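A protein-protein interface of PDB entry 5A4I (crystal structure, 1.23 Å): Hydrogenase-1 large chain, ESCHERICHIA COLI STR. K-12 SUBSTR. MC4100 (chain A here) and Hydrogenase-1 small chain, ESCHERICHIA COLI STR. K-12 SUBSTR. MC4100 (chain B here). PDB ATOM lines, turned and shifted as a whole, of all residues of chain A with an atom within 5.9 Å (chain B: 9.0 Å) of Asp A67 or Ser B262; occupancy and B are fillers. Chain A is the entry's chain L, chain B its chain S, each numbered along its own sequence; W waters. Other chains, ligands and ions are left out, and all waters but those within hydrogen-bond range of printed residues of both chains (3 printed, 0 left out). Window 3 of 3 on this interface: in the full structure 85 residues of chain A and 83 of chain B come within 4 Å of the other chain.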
ATOM      1  N   LEU A  60     -15.447  -3.031 -11.538  1.00  0.00           N
ATOM      2  CA  LEU A  60     -15.234  -3.881 -12.729  1.00  0.00           C
ATOM      3  C   LEU A  60     -14.333  -3.230 -13.787  1.00  0.00           C
ATOM      4  O   LEU A  60     -13.793  -3.915 -14.649  1.00  0.00           O
ATOM      5  CB  LEU A  60     -16.578  -4.248 -13.351  1.00  0.00           C
ATOM      6  CG  LEU A  60     -17.099  -5.590 -12.876  1.00  0.00           C
ATOM      7  CD1 LEU A  60     -16.348  -6.751 -13.433  1.00  0.00           C
ATOM      8  CD2 LEU A  60     -17.159  -5.811 -11.410  1.00  0.00           C
ATOM      9  N   ARG A  63     -10.804  -4.665 -15.234  1.00  0.00           N
ATOM     10  CA  ARG A  63     -10.646  -6.098 -14.956  1.00  0.00           C
ATOM     11  C   ARG A  63     -10.525  -6.847 -16.275  1.00  0.00           C
ATOM     12  O   ARG A  63     -10.996  -6.432 -17.335  1.00  0.00           O
ATOM     13  CB  ARG A  63     -11.805  -6.651 -14.125  1.00  0.00           C
ATOM     14  CG  ARG A  63     -12.081  -5.953 -12.809  1.00  0.00           C
ATOM     15  CD  ARG A  63     -10.933  -6.042 -11.843  1.00  0.00           C
ATOM     16  NE  ARG A  63     -11.145  -5.185 -10.651  1.00  0.00           N
ATOM     17  CZ  ARG A  63     -10.384  -5.253  -9.577  1.00  0.00           C
ATOM     18  NH1 ARG A  63      -9.422  -6.181  -9.511  1.00  0.00           N
ATOM     19  NH2 ARG A  63     -10.597  -4.455  -8.550  1.00  0.00           N
ATOM     20  N   ASP A  64      -9.930  -8.025 -16.175  1.00  0.00           N
ATOM     21  CA  ASP A  64      -9.937  -8.924 -17.333  1.00  0.00           C
ATOM     22  C   ASP A  64     -11.368  -9.441 -17.542  1.00  0.00           C
ATOM     23  O   ASP A  64     -12.034  -9.876 -16.593  1.00  0.00           O
ATOM     24  CB  ASP A  64      -8.961 -10.072 -17.124  1.00  0.00           C
ATOM     25  CG  ASP A  64      -8.739 -10.927 -18.373  1.00  0.00           C
ATOM     26  OD1 ASP A  64      -9.709 -11.546 -18.892  1.00  0.00           O
ATOM     27  OD2 ASP A  64      -7.569 -11.063 -18.778  1.00  0.00           O
ATOM     28  N   PRO A  65     -11.882  -9.373 -18.759  1.00  0.00           N
ATOM     29  CA  PRO A  65     -13.270  -9.833 -19.008  1.00  0.00           C
ATOM     30  C   PRO A  65     -13.560 -11.258 -18.549  1.00  0.00           C
ATOM     31  O   PRO A  65     -14.685 -11.583 -18.231  1.00  0.00           O
ATOM     32  CB  PRO A  65     -13.433  -9.657 -20.525  1.00  0.00           C
ATOM     33  CG  PRO A  65     -12.460  -8.581 -20.870  1.00  0.00           C
ATOM     34  CD  PRO A  65     -11.298  -8.787 -19.974  1.00  0.00           C
ATOM     35  N   ARG A  66     -12.532 -12.110 -18.584  1.00  0.00           N
ATOM     36  CA  ARG A  66     -12.694 -13.478 -18.148  1.00  0.00           C
ATOM     37  C   ARG A  66     -12.967 -13.603 -16.651  1.00  0.00           C
ATOM     38  O   ARG A  66     -13.523 -14.610 -16.213  1.00  0.00           O
ATOM     39  CB  ARG A  66     -11.476 -14.326 -18.503  1.00  0.00           C
ATOM     40  CG  ARG A  66     -11.286 -14.449 -20.019  1.00  0.00           C
ATOM     41  CD  ARG A  66      -9.974 -15.020 -20.428  1.00  0.00           C
ATOM     42  NE  ARG A  66      -8.873 -14.142 -20.080  1.00  0.00           N
ATOM     43  CZ  ARG A  66      -7.600 -14.477 -20.147  1.00  0.00           C
ATOM     44  NH1 ARG A  66      -7.229 -15.647 -20.681  1.00  0.00           N
ATOM     45  NH2 ARG A  66      -6.690 -13.633 -19.710  1.00  0.00           N
ATOM     46  N   ASP A  67     -12.524 -12.605 -15.886  1.00  0.00           N
ATOM     47  CA  ASP A  67     -12.706 -12.572 -14.434  1.00  0.00           C
ATOM     48  C   ASP A  67     -14.034 -11.926 -14.027  1.00  0.00           C
ATOM     49  O   ASP A  67     -14.426 -12.012 -12.864  1.00  0.00           O
ATOM     50  CB  ASP A  67     -11.579 -11.727 -13.796  1.00  0.00           C
ATOM     51  CG  ASP A  67     -10.202 -12.391 -13.839  1.00  0.00           C
ATOM     52  OD1 ASP A  67     -10.076 -13.585 -13.575  1.00  0.00           O
ATOM     53  OD2 ASP A  67      -9.207 -11.703 -14.163  1.00  0.00           O
ATOM     54  N   ALA A  68     -14.706 -11.248 -14.942  1.00  0.00           N
ATOM     55  CA  ALA A  68     -15.813 -10.382 -14.540  1.00  0.00           C
ATOM     56  C   ALA A  68     -16.907 -11.145 -13.812  1.00  0.00           C
ATOM     57  O   ALA A  68     -17.484 -10.621 -12.863  1.00  0.00           O
ATOM     58  CB  ALA A  68     -16.370  -9.650 -15.728  1.00  0.00           C
ATOM     59  N   TRP A  69     -17.212 -12.358 -14.268  1.00  0.00           N
ATOM     60  CA  TRP A  69     -18.316 -13.129 -13.695  1.00  0.00           C
ATOM     61  C   TRP A  69     -18.147 -13.283 -12.187  1.00  0.00           C
ATOM     62  O   TRP A  69     -19.122 -13.305 -11.460  1.00  0.00           O
ATOM     63  CB  TRP A  69     -18.449 -14.512 -14.343  1.00  0.00           C
ATOM     64  CG  TRP A  69     -17.307 -15.421 -14.083  1.00  0.00           C
ATOM     65  CD1 TRP A  69     -16.197 -15.579 -14.843  1.00  0.00           C
ATOM     66  CD2 TRP A  69     -17.111 -16.231 -12.920  1.00  0.00           C
ATOM     67  NE1 TRP A  69     -15.301 -16.411 -14.221  1.00  0.00           N
ATOM     68  CE2 TRP A  69     -15.859 -16.849 -13.049  1.00  0.00           C
ATOM     69  CE3 TRP A  69     -17.878 -16.485 -11.760  1.00  0.00           C
ATOM     70  CZ2 TRP A  69     -15.345 -17.685 -12.075  1.00  0.00           C
ATOM     71  CZ3 TRP A  69     -17.349 -17.299 -10.788  1.00  0.00           C
ATOM     72  CH2 TRP A  69     -16.093 -17.880 -10.940  1.00  0.00           C
ATOM     73  N   ALA A  70     -16.892 -13.431 -11.738  1.00  0.00           N
ATOM     74  CA  ALA A  70     -16.632 -13.728 -10.323  1.00  0.00           C
ATOM     75  C   ALA A  70     -16.910 -12.531  -9.442  1.00  0.00           C
ATOM     76  O   ALA A  70     -17.395 -12.669  -8.309  1.00  0.00           O
ATOM     77  CB  ALA A  70     -15.218 -14.271 -10.123  1.00  0.00           C
ATOM     78  N   PHE A  71     -16.556 -11.342  -9.959  1.00  0.00           N
ATOM     79  CA  PHE A  71     -16.843 -10.090  -9.277  1.00  0.00           C
ATOM     80  C   PHE A  71     -18.329  -9.825  -9.225  1.00  0.00           C
ATOM     81  O   PHE A  71     -18.906  -9.578  -8.173  1.00  0.00           O
ATOM     82  CB  PHE A  71     -16.169  -8.913  -9.984  1.00  0.00           C
ATOM     83  CG  PHE A  71     -14.697  -8.798  -9.781  1.00  0.00           C
ATOM     84  CD1 PHE A  71     -13.797  -9.595 -10.484  1.00  0.00           C
ATOM     85  CD2 PHE A  71     -14.179  -7.832  -8.926  1.00  0.00           C
ATOM     86  CE1 PHE A  71     -12.436  -9.473 -10.284  1.00  0.00           C
ATOM     87  CE2 PHE A  71     -12.817  -7.689  -8.721  1.00  0.00           C
ATOM     88  CZ  PHE A  71     -11.935  -8.515  -9.408  1.00  0.00           C
ATOM     89  N   VAL A  72     -19.008  -9.887 -10.375  1.00  0.00           N
ATOM     90  CA  VAL A  72     -20.427  -9.536 -10.411  1.00  0.00           C
ATOM     91  C   VAL A  72     -21.308 -10.595  -9.783  1.00  0.00           C
ATOM     92  O   VAL A  72     -22.397 -10.271  -9.323  1.00  0.00           O
ATOM     93  CB  VAL A  72     -20.930  -9.115 -11.795  1.00  0.00           C
ATOM     94  CG1 VAL A  72     -20.248  -7.855 -12.267  1.00  0.00           C
ATOM     95  CG2 VAL A  72     -20.803 -10.249 -12.805  1.00  0.00           C
ATOM     96  N   VAL A 234     -16.000 -18.061 -18.945  1.00  0.00           N
ATOM     97  CA  VAL A 234     -16.222 -17.580 -20.322  1.00  0.00           C
ATOM     98  C   VAL A 234     -15.791 -18.705 -21.270  1.00  0.00           C
ATOM     99  O   VAL A 234     -14.650 -19.192 -21.182  1.00  0.00           O
ATOM    100  CB  VAL A 234     -15.420 -16.291 -20.575  1.00  0.00           C
ATOM    101  CG1 VAL A 234     -15.469 -15.905 -22.068  1.00  0.00           C
ATOM    102  CG2 VAL A 234     -15.948 -15.177 -19.695  1.00  0.00           C
ATOM    103  N   VAL B 121     -15.570  -7.728  -1.947  1.00  0.00           N
ATOM    104  CA  VAL B 121     -15.587  -7.202  -3.313  1.00  0.00           C
ATOM    105  C   VAL B 121     -15.752  -5.672  -3.312  1.00  0.00           C
ATOM    106  O   VAL B 121     -15.114  -4.986  -4.126  1.00  0.00           O
ATOM    107  CB  VAL B 121     -16.647  -7.916  -4.175  1.00  0.00           C
ATOM    108  CG1 VAL B 121     -18.056  -7.451  -3.831  1.00  0.00           C
ATOM    109  CG2 VAL B 121     -16.374  -7.750  -5.647  1.00  0.00           C
ATOM    110  N   TRP B 205      -9.211 -25.199 -20.812  1.00  0.00           N
ATOM    111  CA  TRP B 205     -10.431 -25.828 -20.326  1.00  0.00           C
ATOM    112  C   TRP B 205     -10.845 -27.027 -21.175  1.00  0.00           C
ATOM    113  O   TRP B 205     -10.806 -26.984 -22.414  1.00  0.00           O
ATOM    114  CB  TRP B 205     -11.592 -24.858 -20.238  1.00  0.00           C
ATOM    115  CG  TRP B 205     -11.258 -23.631 -19.484  1.00  0.00           C
ATOM    116  CD1 TRP B 205     -11.243 -22.378 -19.980  1.00  0.00           C
ATOM    117  CD2 TRP B 205     -10.985 -23.511 -18.079  1.00  0.00           C
ATOM    118  NE1 TRP B 205     -10.903 -21.484 -18.994  1.00  0.00           N
ATOM    119  CE2 TRP B 205     -10.733 -22.148 -17.826  1.00  0.00           C
ATOM    120  CE3 TRP B 205     -10.923 -24.429 -17.003  1.00  0.00           C
ATOM    121  CZ2 TRP B 205     -10.415 -21.677 -16.577  1.00  0.00           C
ATOM    122  CZ3 TRP B 205     -10.598 -23.964 -15.759  1.00  0.00           C
ATOM    123  CH2 TRP B 205     -10.340 -22.596 -15.554  1.00  0.00           C
ATOM    124  N   TYR B 217      -3.208 -25.443 -11.232  1.00  0.00           N
ATOM    125  CA  TYR B 217      -2.206 -24.360 -10.992  1.00  0.00           C
ATOM    126  C   TYR B 217      -2.003 -23.458 -12.203  1.00  0.00           C
ATOM    127  O   TYR B 217      -1.965 -22.235 -12.080  1.00  0.00           O
ATOM    128  CB  TYR B 217      -0.902 -25.042 -10.560  1.00  0.00           C
ATOM    129  CG  TYR B 217       0.247 -24.086 -10.483  1.00  0.00           C
ATOM    130  CD1 TYR B 217       0.356 -23.152  -9.461  1.00  0.00           C
ATOM    131  CD2 TYR B 217       1.224 -24.115 -11.466  1.00  0.00           C
ATOM    132  CE1 TYR B 217       1.427 -22.240  -9.418  1.00  0.00           C
ATOM    133  CE2 TYR B 217       2.290 -23.224 -11.448  1.00  0.00           C
ATOM    134  CZ  TYR B 217       2.418 -22.248 -10.421  1.00  0.00           C
ATOM    135  OH  TYR B 217       3.468 -21.392 -10.382  1.00  0.00           O
ATOM    136  N   MET B 219      -4.022 -22.909 -14.566  1.00  0.00           N
ATOM    137  CA  MET B 219      -5.280 -22.201 -14.798  1.00  0.00           C
ATOM    138  C   MET B 219      -5.531 -21.127 -13.737  1.00  0.00           C
ATOM    139  O   MET B 219      -6.618 -20.506 -13.756  1.00  0.00           O
ATOM    140  CB  MET B 219      -6.476 -23.181 -14.875  1.00  0.00           C
ATOM    141  CG  MET B 219      -6.270 -24.239 -15.935  1.00  0.00           C
ATOM    142  SD  MET B 219      -5.843 -23.656 -17.595  1.00  0.00           S
ATOM    143  CE  MET B 219      -7.260 -22.621 -18.025  1.00  0.00           C
ATOM    144  N   GLY B 220      -4.546 -20.855 -12.861  1.00  0.00           N
ATOM    145  CA  GLY B 220      -4.664 -19.757 -11.935  1.00  0.00           C
ATOM    146  C   GLY B 220      -5.041 -20.129 -10.500  1.00  0.00           C
ATOM    147  O   GLY B 220      -5.286 -19.241  -9.674  1.00  0.00           O
ATOM    148  N   CYS B 221      -5.129 -21.420 -10.170  1.00  0.00           N
ATOM    149  CA  CYS B 221      -5.553 -21.818  -8.833  1.00  0.00           C
ATOM    150  C   CYS B 221      -4.735 -21.109  -7.760  1.00  0.00           C
ATOM    151  O   CYS B 221      -3.501 -21.178  -7.768  1.00  0.00           O
ATOM    152  CB  CYS B 221      -5.350 -23.332  -8.651  1.00  0.00           C
ATOM    153  SG  CYS B 221      -5.990 -23.925  -7.089  1.00  0.00           S
ATOM    154  N   LYS B 222      -5.413 -20.493  -6.783  1.00  0.00           N
ATOM    155  CA  LYS B 222      -4.783 -19.816  -5.665  1.00  0.00           C
ATOM    156  C   LYS B 222      -4.739 -20.648  -4.381  1.00  0.00           C
ATOM    157  O   LYS B 222      -4.409 -20.140  -3.301  1.00  0.00           O
ATOM    158  CB  LYS B 222      -5.444 -18.432  -5.442  1.00  0.00           C
ATOM    159  CG  LYS B 222      -5.319 -17.522  -6.709  1.00  0.00           C
ATOM    160  CD  LYS B 222      -3.889 -17.490  -7.297  1.00  0.00           C
ATOM    161  CE  LYS B 222      -3.635 -16.520  -8.412  1.00  0.00           C
ATOM    162  NZ  LYS B 222      -4.632 -16.491  -9.479  1.00  0.00           N
ATOM    163  N   HIS B 247     -12.637 -25.679 -11.314  1.00  0.00           N
ATOM    164  CA  HIS B 247     -12.165 -24.306 -11.329  1.00  0.00           C
ATOM    165  C   HIS B 247     -11.126 -24.126 -10.241  1.00  0.00           C
ATOM    166  O   HIS B 247     -11.303 -24.622  -9.123  1.00  0.00           O
ATOM    167  CB  HIS B 247     -13.316 -23.301 -11.137  1.00  0.00           C
ATOM    168  CG  HIS B 247     -12.982 -21.914 -11.590  1.00  0.00           C
ATOM    169  ND1 HIS B 247     -12.108 -21.084 -10.940  1.00  0.00           N
ATOM    170  CD2 HIS B 247     -13.412 -21.215 -12.662  1.00  0.00           C
ATOM    171  CE1 HIS B 247     -11.991 -19.948 -11.621  1.00  0.00           C
ATOM    172  NE2 HIS B 247     -12.761 -20.010 -12.678  1.00  0.00           N
ATOM    173  N   CYS B 249      -9.100 -22.479  -7.194  1.00  0.00           N
ATOM    174  CA  CYS B 249      -9.418 -21.591  -6.085  1.00  0.00           C
ATOM    175  C   CYS B 249      -9.158 -20.122  -6.523  1.00  0.00           C
ATOM    176  O   CYS B 249      -8.158 -19.825  -7.173  1.00  0.00           O
ATOM    177  CB  CYS B 249      -8.546 -21.988  -4.905  1.00  0.00           C
ATOM    178  SG  CYS B 249      -8.645 -20.972  -3.406  1.00  0.00           S
ATOM    179  N   LEU B 250     -10.094 -19.250  -6.178  1.00  0.00           N
ATOM    180  CA  LEU B 250      -9.958 -17.819  -6.403  1.00  0.00           C
ATOM    181  C   LEU B 250      -9.156 -17.135  -5.314  1.00  0.00           C
ATOM    182  O   LEU B 250      -8.759 -15.964  -5.461  1.00  0.00           O
ATOM    183  CB  LEU B 250     -11.326 -17.144  -6.443  1.00  0.00           C
ATOM    184  CG  LEU B 250     -12.396 -17.707  -7.345  1.00  0.00           C
ATOM    185  CD1 LEU B 250     -13.716 -16.964  -7.191  1.00  0.00           C
ATOM    186  CD2 LEU B 250     -11.957 -17.692  -8.803  1.00  0.00           C
ATOM    187  N   GLY B 251      -8.968 -17.813  -4.178  1.00  0.00           N
ATOM    188  CA  GLY B 251      -8.344 -17.218  -3.009  1.00  0.00           C
ATOM    189  C   GLY B 251      -9.298 -16.525  -2.069  1.00  0.00           C
ATOM    190  O   GLY B 251      -8.861 -15.669  -1.295  1.00  0.00           O
ATOM    191  N   PHE B 257      -7.979 -10.649  -1.995  1.00  0.00           N
ATOM    192  CA  PHE B 257      -7.862 -11.647  -3.081  1.00  0.00           C
ATOM    193  C   PHE B 257      -8.341 -11.135  -4.414  1.00  0.00           C
ATOM    194  O   PHE B 257      -7.851 -11.596  -5.439  1.00  0.00           O
ATOM    195  CB  PHE B 257      -8.555 -12.979  -2.722  1.00  0.00           C
ATOM    196  CG  PHE B 257     -10.063 -12.991  -2.832  1.00  0.00           C
ATOM    197  CD1 PHE B 257     -10.831 -12.504  -1.808  1.00  0.00           C
ATOM    198  CD2 PHE B 257     -10.674 -13.470  -3.977  1.00  0.00           C
ATOM    199  CE1 PHE B 257     -12.230 -12.540  -1.904  1.00  0.00           C
ATOM    200  CE2 PHE B 257     -12.067 -13.530  -4.086  1.00  0.00           C
ATOM    201  CZ  PHE B 257     -12.832 -13.086  -3.034  1.00  0.00           C
ATOM    202  N   TRP B 258      -9.242 -10.150  -4.426  1.00  0.00           N
ATOM    203  CA  TRP B 258      -9.736  -9.595  -5.681  1.00  0.00           C
ATOM    204  C   TRP B 258      -8.657  -8.839  -6.468  1.00  0.00           C
ATOM    205  O   TRP B 258      -8.782  -8.707  -7.679  1.00  0.00           O
ATOM    206  CB  TRP B 258     -10.891  -8.642  -5.443  1.00  0.00           C
ATOM    207  CG  TRP B 258     -12.081  -9.285  -4.774  1.00  0.00           C
ATOM    208  CD1 TRP B 258     -12.461  -9.216  -3.452  1.00  0.00           C
ATOM    209  CD2 TRP B 258     -13.079 -10.106  -5.419  1.00  0.00           C
ATOM    210  NE1 TRP B 258     -13.598  -9.929  -3.265  1.00  0.00           N
ATOM    211  CE2 TRP B 258     -14.009 -10.490  -4.433  1.00  0.00           C
ATOM    212  CE3 TRP B 258     -13.257 -10.569  -6.711  1.00  0.00           C
ATOM    213  CZ2 TRP B 258     -15.084 -11.310  -4.691  1.00  0.00           C
ATOM    214  CZ3 TRP B 258     -14.338 -11.415  -6.964  1.00  0.00           C
ATOM    215  CH2 TRP B 258     -15.233 -11.760  -5.950  1.00  0.00           C
ATOM    216  N   ASP B 259      -7.667  -8.324  -5.769  1.00  0.00           N
ATOM    217  CA  ASP B 259      -6.669  -7.435  -6.351  1.00  0.00           C
ATOM    218  C   ASP B 259      -5.287  -8.088  -6.437  1.00  0.00           C
ATOM    219  O   ASP B 259      -4.304  -7.397  -6.677  1.00  0.00           O
ATOM    220  CB  ASP B 259      -6.636  -6.113  -5.600  1.00  0.00           C
ATOM    221  CG  ASP B 259      -7.874  -5.289  -5.821  1.00  0.00           C
ATOM    222  OD1 ASP B 259      -8.416  -5.235  -6.923  1.00  0.00           O
ATOM    223  OD2 ASP B 259      -8.295  -4.568  -4.870  1.00  0.00           O
ATOM    224  N   ARG B 260      -5.232  -9.396  -6.360  1.00  0.00           N
ATOM    225  CA  ARG B 260      -3.964 -10.146  -6.553  1.00  0.00           C
ATOM    226  C   ARG B 260      -3.752 -10.588  -7.996  1.00  0.00           C
ATOM    227  O   ARG B 260      -3.085 -11.633  -8.268  1.00  0.00           O
ATOM    228  CB  ARG B 260      -4.030 -11.420  -5.732  1.00  0.00           C
ATOM    229  CG  ARG B 260      -3.964 -11.143  -4.318  1.00  0.00           C
ATOM    230  CD  ARG B 260      -2.646 -11.601  -3.665  1.00  0.00           C
ATOM    231  NE  ARG B 260      -2.669 -10.877  -2.398  1.00  0.00           N
ATOM    232  CZ  ARG B 260      -3.616 -11.005  -1.447  1.00  0.00           C
ATOM    233  NH1 ARG B 260      -4.680 -11.942  -1.473  1.00  0.00           N
ATOM    234  NH2 ARG B 260      -3.473 -10.181  -0.394  1.00  0.00           N
ATOM    235  N   GLY B 261      -4.217  -9.844  -8.953  1.00  0.00           N
ATOM    236  CA  GLY B 261      -4.151 -10.235 -10.324  1.00  0.00           C
ATOM    237  C   GLY B 261      -5.315 -11.119 -10.720  1.00  0.00           C
ATOM    238  O   GLY B 261      -6.159 -11.559  -9.909  1.00  0.00           O
ATOM    239  N   SER B 262      -5.338 -11.396 -11.997  1.00  0.00           N
ATOM    240  CA  SER B 262      -6.403 -12.192 -12.628  1.00  0.00           C
ATOM    241  C   SER B 262      -6.494 -13.524 -11.936  1.00  0.00           C
ATOM    242  O   SER B 262      -5.484 -14.151 -11.578  1.00  0.00           O
ATOM    243  CB  SER B 262      -6.156 -12.423 -14.123  1.00  0.00           C
ATOM    244  OG  SER B 262      -7.147 -13.357 -14.738  1.00  0.00           O
ATOM    245  N   PHE B 263      -7.721 -14.007 -11.789  1.00  0.00           N
ATOM    246  CA  PHE B 263      -7.900 -15.362 -11.276  1.00  0.00           C
ATOM    247  C   PHE B 263      -7.256 -16.413 -12.132  1.00  0.00           C
ATOM    248  O   PHE B 263      -7.003 -17.501 -11.635  1.00  0.00           O
ATOM    249  CB  PHE B 263      -9.394 -15.654 -11.094  1.00  0.00           C
ATOM    250  CG  PHE B 263     -10.036 -14.734 -10.069  1.00  0.00           C
ATOM    251  CD1 PHE B 263      -9.499 -14.653  -8.790  1.00  0.00           C
ATOM    252  CD2 PHE B 263     -11.145 -13.976 -10.386  1.00  0.00           C
ATOM    253  CE1 PHE B 263     -10.037 -13.810  -7.834  1.00  0.00           C
ATOM    254  CE2 PHE B 263     -11.715 -13.155  -9.416  1.00  0.00           C
ATOM    255  CZ  PHE B 263     -11.153 -13.107  -8.164  1.00  0.00           C
ATOM    256  N   TYR B 264      -6.983 -16.092 -13.405  1.00  0.00           N
ATOM    257  CA  TYR B 264      -6.433 -17.049 -14.318  1.00  0.00           C
ATOM    258  C   TYR B 264      -4.938 -16.890 -14.531  1.00  0.00           C
ATOM    259  O   TYR B 264      -4.347 -17.646 -15.297  1.00  0.00           O
ATOM    260  CB  TYR B 264      -7.210 -17.050 -15.661  1.00  0.00           C
ATOM    261  CG  TYR B 264      -8.665 -17.300 -15.390  1.00  0.00           C
ATOM    262  CD1 TYR B 264      -9.093 -18.539 -14.979  1.00  0.00           C
ATOM    263  CD2 TYR B 264      -9.581 -16.300 -15.501  1.00  0.00           C
ATOM    264  CE1 TYR B 264     -10.389 -18.754 -14.642  1.00  0.00           C
ATOM    265  CE2 TYR B 264     -10.920 -16.497 -15.190  1.00  0.00           C
ATOM    266  CZ  TYR B 264     -11.331 -17.745 -14.790  1.00  0.00           C
ATOM    267  OH  TYR B 264     -12.670 -18.001 -14.515  1.00  0.00           O
ATOM    268  N   SER B 265      -4.297 -16.006 -13.759  1.00  0.00           N
ATOM    269  CA  SER B 265      -2.832 -15.873 -13.755  1.00  0.00           C
ATOM    270  C   SER B 265      -2.257 -16.685 -12.609  1.00  0.00           C
ATOM    271  O   SER B 265      -2.821 -16.728 -11.547  1.00  0.00           O
ATOM    272  CB  SER B 265      -2.447 -14.450 -13.545  1.00  0.00           C
ATOM    273  OG  SER B 265      -2.819 -13.736 -14.680  1.00  0.00           O
ATOM    274  N   ARG B 266      -1.135 -17.364 -12.844  1.00  0.00           N
ATOM    275  CA  ARG B 266      -0.518 -18.295 -11.876  1.00  0.00           C
ATOM    276  C   ARG B 266      -0.083 -17.621 -10.611  1.00  0.00           C
ATOM    277  O   ARG B 266       0.370 -16.469 -10.683  1.00  0.00           O
ATOM    278  CB  ARG B 266       0.725 -18.947 -12.476  1.00  0.00           C
ATOM    279  CG  ARG B 266       0.408 -19.781 -13.662  1.00  0.00           C
ATOM    280  CD  ARG B 266       1.689 -20.373 -14.213  1.00  0.00           C
ATOM    281  NE  ARG B 266       1.463 -20.768 -15.580  1.00  0.00           N
ATOM    282  CZ  ARG B 266       2.338 -21.448 -16.306  1.00  0.00           C
ATOM    283  NH1 ARG B 266       3.500 -21.827 -15.767  1.00  0.00           N
ATOM    284  NH2 ARG B 266       2.042 -21.760 -17.557  1.00  0.00           N
ATOM    285  N   VAL B 267      -0.179 -18.355  -9.467  1.00  0.00           N
ATOM    286  CA  VAL B 267       0.362 -17.892  -8.152  1.00  0.00           C
ATOM    287  C   VAL B 267       1.796 -17.469  -8.362  1.00  0.00           C
ATOM    288  O   VAL B 267       2.559 -18.298  -8.851  1.00  0.00           O
ATOM    289  CB  VAL B 267       0.373 -19.007  -7.007  1.00  0.00           C
ATOM    290  CG1 VAL B 267       1.525 -18.822  -5.976  1.00  0.00           C
ATOM    291  CG2 VAL B 267      -0.900 -19.036  -6.171  1.00  0.00           C
HETATM  292  O   HOH W   1      -5.292 -13.973 -16.620  1.00  0.00           O
HETATM  293  O   HOH W   2      -8.470  -8.388 -11.123  1.00  0.00           O
HETATM  294  O   HOH W   3     -13.757 -17.190 -17.240  1.00  0.00           O
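Water W1 lies within hydrogen-bond range of OG of Ser B262 (2.7 Å), OG of Ser B265 (3.2 Å) and NH2 of Arg A66 (3.4 Å).
Water W3 lies within hydrogen-bond range of O of Arg A66, N of Val A234, OH of Tyr B264 and NE1 of Trp A69.
Water W2 lies within hydrogen-bond range of NH1 of Arg A63 (2.9 Å) and O of Trp B258 (3.5 Å).
Printed residues of chain B within 4 Å of Asp A67: Ser B262, Phe B263 and Tyr B264.
Of the printed residues of chain B, Ala A70 touches Trp B258 and Phe B263.
Trp B205 touches none of the printed residues of chain A.
Leu B250 touches none of the printed residues of chain A.
Of the printed residues of chain A, Trp B258 touches Arg A63 (3.2 Å), Ala A70 (3.3 Å) and Phe A71 (3.5 Å).
Of the printed residues of chain A, Phe B263 touches Asp A67 (3.0 Å), Ala A70 (3.7 Å) and Phe A71 (3.9 Å).
The nearest printed residue of chain A that does not touch Ser B262 is Asp A64 (4.4 Å).
Hydrophobic or aromatic side chains of chain A within 4 Å of the printed part of chain B: Trp A69, Ala A70 and Phe A71.
Along chain B the printed residues that touch a printed residue of chain A span positions 121 to 264.
OD2 of Asp A64 lies within salt-bridge range of NH2 of Arg A66 (2.9 Å).
O of Arg A66 sits close to NE1 of Trp A69, 3.2 Å away.
The side-chain amino group (NZ) of Lys B222 lies within hydrogen-bond range of the backbone carbonyl oxygen (O) of Ser B262, at 3.3 Å.
O of Phe B263 is in hydrogen-bond range of NZ of Lys B222 (3.4 Å).
The side-chain hydroxyl (OH) of Tyr B264 sits at hydrogen-bond distance from a ring nitrogen (NE2) of His B247, 2.7 Å away.
N of Tyr B264 sits close to OG of Ser B262.
Among the printed residues, merely in contact across the chains: Ala A70 with Trp B258, Asp A67 with Tyr B264, Arg A66 with Tyr B264, Trp A69 with His B247, Phe A71 with Trp B258, Ala A70 with Phe B263, Phe A71 with Phe B263 and Phe A71 with Val B121.
The guanidinium group of Arg A63 lies within hydrogen-bond range of the backbone carbonyl oxygen of Trp B258 (3.2 Å).
OD1 of Asp B259 lies within salt-bridge range of NH2 of Arg A63 (2.8 Å).
The side-chain carboxylate (OD2) of Asp A67 is in hydrogen-bond range of the side-chain hydroxyl (OG) of Ser B262, 2.7 Å away.
The side-chain carboxylate (OD1) of Asp A67 lies within hydrogen-bond range of the backbone NH (N) of Phe B263, at 3.0 Å.
The indole nitrogen (NE1) of Trp A69 sits at hydrogen-bond distance from the side-chain hydroxyl (OH) of Tyr B264.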
